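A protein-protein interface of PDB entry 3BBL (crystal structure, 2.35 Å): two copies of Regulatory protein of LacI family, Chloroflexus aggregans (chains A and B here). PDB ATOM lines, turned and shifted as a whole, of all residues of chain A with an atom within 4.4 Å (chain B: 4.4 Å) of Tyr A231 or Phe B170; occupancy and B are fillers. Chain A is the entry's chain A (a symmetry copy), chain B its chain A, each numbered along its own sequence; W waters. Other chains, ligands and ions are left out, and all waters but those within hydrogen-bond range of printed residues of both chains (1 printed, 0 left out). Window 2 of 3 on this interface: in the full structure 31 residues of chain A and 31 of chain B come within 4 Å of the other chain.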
ATOM      1  N   MET A 228      11.600 -11.967  26.041  1.00  0.00           N
ATOM      2  CA  MET A 228      12.441 -10.866  25.598  1.00  0.00           C
ATOM      3  C   MET A 228      11.971 -10.081  24.377  1.00  0.00           C
ATOM      4  O   MET A 228      12.441  -8.961  24.159  1.00  0.00           O
ATOM      5  CB  MET A 228      13.863 -11.330  25.327  1.00  0.00           C
ATOM      6  CG  MET A 228      14.170 -11.470  23.865  1.00  0.00           C
ATOM      7  SD  MET A 228      16.045 -10.824  23.412  1.00  0.00           S
ATOM      8  CE  MET A 228      15.567  -8.948  23.252  1.00  0.00           C
ATOM      9  N   VAL A 229      11.083 -10.643  23.559  1.00  0.00           N
ATOM     10  CA  VAL A 229      10.636  -9.866  22.412  1.00  0.00           C
ATOM     11  C   VAL A 229      10.001  -8.579  22.944  1.00  0.00           C
ATOM     12  O   VAL A 229       9.954  -7.564  22.259  1.00  0.00           O
ATOM     13  CB  VAL A 229       9.620 -10.646  21.523  1.00  0.00           C
ATOM     14  CG1 VAL A 229      10.258 -11.939  21.030  1.00  0.00           C
ATOM     15  CG2 VAL A 229       8.339 -10.935  22.278  1.00  0.00           C
ATOM     16  N   GLN A 230       9.544  -8.640  24.188  1.00  0.00           N
ATOM     17  CA  GLN A 230       8.926  -7.508  24.861  1.00  0.00           C
ATOM     18  C   GLN A 230       9.950  -6.401  25.158  1.00  0.00           C
ATOM     19  O   GLN A 230       9.585  -5.252  25.396  1.00  0.00           O
ATOM     20  CB  GLN A 230       8.321  -7.992  26.171  1.00  0.00           C
ATOM     21  CG  GLN A 230       9.325  -8.813  26.968  1.00  0.00           C
ATOM     22  CD  GLN A 230       8.769  -9.330  28.267  1.00  0.00           C
ATOM     23  OE1 GLN A 230       9.334 -10.231  28.880  1.00  0.00           O
ATOM     24  NE2 GLN A 230       7.656  -8.760  28.701  1.00  0.00           N
ATOM     25  N   TYR A 231      11.228  -6.755  25.154  1.00  0.00           N
ATOM     26  CA  TYR A 231      12.281  -5.784  25.441  1.00  0.00           C
ATOM     27  C   TYR A 231      12.889  -5.122  24.206  1.00  0.00           C
ATOM     28  O   TYR A 231      13.751  -4.245  24.333  1.00  0.00           O
ATOM     29  CB  TYR A 231      13.406  -6.439  26.252  1.00  0.00           C
ATOM     30  CG  TYR A 231      12.945  -7.074  27.539  1.00  0.00           C
ATOM     31  CD1 TYR A 231      13.352  -8.365  27.877  1.00  0.00           C
ATOM     32  CD2 TYR A 231      12.090  -6.402  28.406  1.00  0.00           C
ATOM     33  CE1 TYR A 231      12.915  -8.979  29.047  1.00  0.00           C
ATOM     34  CE2 TYR A 231      11.647  -7.001  29.578  1.00  0.00           C
ATOM     35  CZ  TYR A 231      12.065  -8.292  29.889  1.00  0.00           C
ATOM     36  OH  TYR A 231      11.629  -8.903  31.031  1.00  0.00           O
ATOM     37  N   LEU A 232      12.452  -5.534  23.021  1.00  0.00           N
ATOM     38  CA  LEU A 232      12.979  -4.961  21.792  1.00  0.00           C
ATOM     39  C   LEU A 232      12.436  -3.549  21.593  1.00  0.00           C
ATOM     40  O   LEU A 232      11.521  -3.133  22.290  1.00  0.00           O
ATOM     41  CB  LEU A 232      12.578  -5.831  20.606  1.00  0.00           C
ATOM     42  CG  LEU A 232      13.018  -7.296  20.638  1.00  0.00           C
ATOM     43  CD1 LEU A 232      12.233  -8.100  19.615  1.00  0.00           C
ATOM     44  CD2 LEU A 232      14.512  -7.390  20.378  1.00  0.00           C
ATOM     45  N   PHE A 233      13.013  -2.803  20.664  1.00  0.00           N
ATOM     46  CA  PHE A 233      12.503  -1.469  20.380  1.00  0.00           C
ATOM     47  C   PHE A 233      12.184  -1.347  18.899  1.00  0.00           C
ATOM     48  O   PHE A 233      13.067  -1.419  18.057  1.00  0.00           O
ATOM     49  CB  PHE A 233      13.502  -0.376  20.748  1.00  0.00           C
ATOM     50  CG  PHE A 233      12.971   1.007  20.501  1.00  0.00           C
ATOM     51  CD1 PHE A 233      11.955   1.526  21.303  1.00  0.00           C
ATOM     52  CD2 PHE A 233      13.423   1.757  19.415  1.00  0.00           C
ATOM     53  CE1 PHE A 233      11.386   2.778  21.027  1.00  0.00           C
ATOM     54  CE2 PHE A 233      12.863   3.006  19.128  1.00  0.00           C
ATOM     55  CZ  PHE A 233      11.838   3.518  19.937  1.00  0.00           C
ATOM     56  N   GLY B  17      10.067 -13.297  32.332  1.00  0.00           N
ATOM     57  CA  GLY B  17      10.760 -12.078  31.961  1.00  0.00           C
ATOM     58  C   GLY B  17      12.248 -12.284  31.768  1.00  0.00           C
ATOM     59  O   GLY B  17      12.973 -11.338  31.461  1.00  0.00           O
ATOM     60  N   THR B 169      17.224  -8.228  36.323  1.00  0.00           N
ATOM     61  CA  THR B 169      16.092  -8.010  35.425  1.00  0.00           C
ATOM     62  C   THR B 169      16.365  -6.887  34.431  1.00  0.00           C
ATOM     63  O   THR B 169      17.331  -6.123  34.560  1.00  0.00           O
ATOM     64  CB  THR B 169      14.798  -7.632  36.193  1.00  0.00           C
ATOM     65  OG1 THR B 169      14.979  -6.371  36.855  1.00  0.00           O
ATOM     66  CG2 THR B 169      14.438  -8.714  37.205  1.00  0.00           C
ATOM     67  N   PHE B 170      15.502  -6.800  33.428  1.00  0.00           N
ATOM     68  CA  PHE B 170      15.594  -5.761  32.413  1.00  0.00           C
ATOM     69  C   PHE B 170      15.398  -4.401  33.085  1.00  0.00           C
ATOM     70  O   PHE B 170      16.174  -3.473  32.876  1.00  0.00           O
ATOM     71  CB  PHE B 170      14.498  -5.963  31.375  1.00  0.00           C
ATOM     72  CG  PHE B 170      14.327  -4.806  30.447  1.00  0.00           C
ATOM     73  CD1 PHE B 170      15.131  -4.678  29.314  1.00  0.00           C
ATOM     74  CD2 PHE B 170      13.375  -3.822  30.715  1.00  0.00           C
ATOM     75  CE1 PHE B 170      14.983  -3.591  28.459  1.00  0.00           C
ATOM     76  CE2 PHE B 170      13.223  -2.731  29.865  1.00  0.00           C
ATOM     77  CZ  PHE B 170      14.031  -2.617  28.738  1.00  0.00           C
ATOM     78  N   GLU B 171      14.351  -4.311  33.898  1.00  0.00           N
ATOM     79  CA  GLU B 171      14.002  -3.092  34.619  1.00  0.00           C
ATOM     80  C   GLU B 171      15.158  -2.594  35.487  1.00  0.00           C
ATOM     81  O   GLU B 171      15.466  -1.397  35.507  1.00  0.00           O
ATOM     82  CB  GLU B 171      12.772  -3.326  35.510  1.00  0.00           C
ATOM     83  CG  GLU B 171      11.477  -3.755  34.800  1.00  0.00           C
ATOM     84  CD  GLU B 171      11.558  -5.116  34.073  1.00  0.00           C
ATOM     85  OE1 GLU B 171      12.278  -6.040  34.532  1.00  0.00           O
ATOM     86  OE2 GLU B 171      10.865  -5.261  33.040  1.00  0.00           O
ATOM     87  N   VAL B 172      15.797  -3.502  36.215  1.00  0.00           N
ATOM     88  CA  VAL B 172      16.909  -3.087  37.059  1.00  0.00           C
ATOM     89  C   VAL B 172      18.107  -2.678  36.203  1.00  0.00           C
ATOM     90  O   VAL B 172      18.754  -1.666  36.474  1.00  0.00           O
ATOM     91  CB  VAL B 172      17.311  -4.202  38.060  1.00  0.00           C
ATOM     92  CG1 VAL B 172      18.619  -3.853  38.752  1.00  0.00           C
ATOM     93  CG2 VAL B 172      16.214  -4.369  39.094  1.00  0.00           C
ATOM     94  N   GLY B 173      18.391  -3.458  35.164  1.00  0.00           N
ATOM     95  CA  GLY B 173      19.507  -3.135  34.290  1.00  0.00           C
ATOM     96  C   GLY B 173      19.350  -1.758  33.671  1.00  0.00           C
ATOM     97  O   GLY B 173      20.301  -0.987  33.591  1.00  0.00           O
ATOM     98  N   ARG B 174      18.131  -1.444  33.252  1.00  0.00           N
ATOM     99  CA  ARG B 174      17.838  -0.157  32.646  1.00  0.00           C
ATOM    100  C   ARG B 174      17.967   0.976  33.664  1.00  0.00           C
ATOM    101  O   ARG B 174      18.643   1.979  33.414  1.00  0.00           O
ATOM    102  CB  ARG B 174      16.426  -0.178  32.058  1.00  0.00           C
ATOM    103  CG  ARG B 174      15.944   1.134  31.480  1.00  0.00           C
ATOM    104  CD  ARG B 174      14.535   0.958  30.922  1.00  0.00           C
ATOM    105  NE  ARG B 174      13.921   2.229  30.553  1.00  0.00           N
ATOM    106  CZ  ARG B 174      13.401   3.095  31.419  1.00  0.00           C
ATOM    107  NH1 ARG B 174      13.409   2.830  32.720  1.00  0.00           N
ATOM    108  NH2 ARG B 174      12.888   4.243  30.988  1.00  0.00           N
ATOM    109  N   THR B 198      19.767 -10.304  30.301  1.00  0.00           N
ATOM    110  CA  THR B 198      18.547  -9.539  30.544  1.00  0.00           C
ATOM    111  C   THR B 198      18.920  -8.131  31.008  1.00  0.00           C
ATOM    112  O   THR B 198      18.338  -7.147  30.554  1.00  0.00           O
ATOM    113  CB  THR B 198      17.676 -10.204  31.613  1.00  0.00           C
ATOM    114  OG1 THR B 198      17.534 -11.592  31.300  1.00  0.00           O
ATOM    115  CG2 THR B 198      16.305  -9.568  31.647  1.00  0.00           C
ATOM    116  N   ILE B 201      20.297  -5.994  28.210  1.00  0.00           N
ATOM    117  CA  ILE B 201      19.270  -5.483  27.316  1.00  0.00           C
ATOM    118  C   ILE B 201      18.687  -4.192  27.886  1.00  0.00           C
ATOM    119  O   ILE B 201      18.430  -3.230  27.147  1.00  0.00           O
ATOM    120  CB  ILE B 201      18.180  -6.557  27.061  1.00  0.00           C
ATOM    121  CG1 ILE B 201      18.798  -7.700  26.242  1.00  0.00           C
ATOM    122  CG2 ILE B 201      17.008  -5.965  26.293  1.00  0.00           C
ATOM    123  CD1 ILE B 201      17.861  -8.850  25.933  1.00  0.00           C
ATOM    124  N   GLY B 202      18.505  -4.161  29.203  1.00  0.00           N
ATOM    125  CA  GLY B 202      17.992  -2.965  29.846  1.00  0.00           C
ATOM    126  C   GLY B 202      18.984  -1.826  29.656  1.00  0.00           C
ATOM    127  O   GLY B 202      18.602  -0.682  29.411  1.00  0.00           O
ATOM    128  N   ALA B 205      18.661  -0.505  26.309  1.00  0.00           N
ATOM    129  CA  ALA B 205      17.463   0.320  26.219  1.00  0.00           C
ATOM    130  C   ALA B 205      17.735   1.710  26.795  1.00  0.00           C
ATOM    131  O   ALA B 205      17.265   2.718  26.264  1.00  0.00           O
ATOM    132  CB  ALA B 205      16.321  -0.343  26.968  1.00  0.00           C
HETATM  133  O   HOH W   1      13.270  -8.522  33.341  1.00  0.00           O
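The backbone carbonyl oxygen of Gly B17 sits at hydrogen-bond distance from the side-chain hydroxyl of Tyr A231 (2.8 Å).
The side-chain amide oxygen (OE1) of Gln A230 is in hydrogen-bond range of the side-chain hydroxyl (OH) of Tyr A231 (3.4 Å).
Met A228 touches Ile B201 (CE to CD1, 3.5 Å).
Gln A230 touches Gly B17.
CG of Phe B170 touches CD2 of Tyr A231 (3.4 Å).
OE2 of Glu B171 touches CE2 of Tyr A231 (3.95 Å).
Tyr A231 touches Ile B201.
Of the printed residues of chain B, Met A228 touches Ile B201.
Val A229 touches none of the printed residues of chain B.
Printed residues of chain B within 4 Å of Gln A230: Gly B17 (3.9 Å).
Leu A232 touches none of the printed residues of chain B.
Of the printed residues of chain A, Gly B17 touches Gln A230 and Tyr A231.
Of chain A, only Tyr A231 (3.4 Å) comes within 4 Å of Phe B170.
Of the printed residues of chain A, Ile B201 touches Met A228 (3.5 Å) and Tyr A231 (3.6 Å).
The nearest residue of chain B that does not touch Tyr A231 is Thr B198 (4.3 Å).
Hydrophobic or aromatic side chains of chain A that line the printed part of chain B: Met A228 and Tyr A231.
Printed residues of chain B that touch a printed residue of chain A: Gly B17, Phe B170, Glu B171 and Ile B201.
Along chain B the printed residues that touch a printed residue of chain A span positions 17 to 201.
Among the printed residues, no Asp or Glu carboxylate lies within 4 Å of a Lys or Arg side-chain nitrogen of the other chain.
No position is printed for both chains.
Water W1 lies within hydrogen-bond range of N of Phe B170 (2.8 Å), OH of Tyr A231 (2.9 Å), OE1 of Glu B171 (2.9 Å) and O of Gly B17 (3.4 Å).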
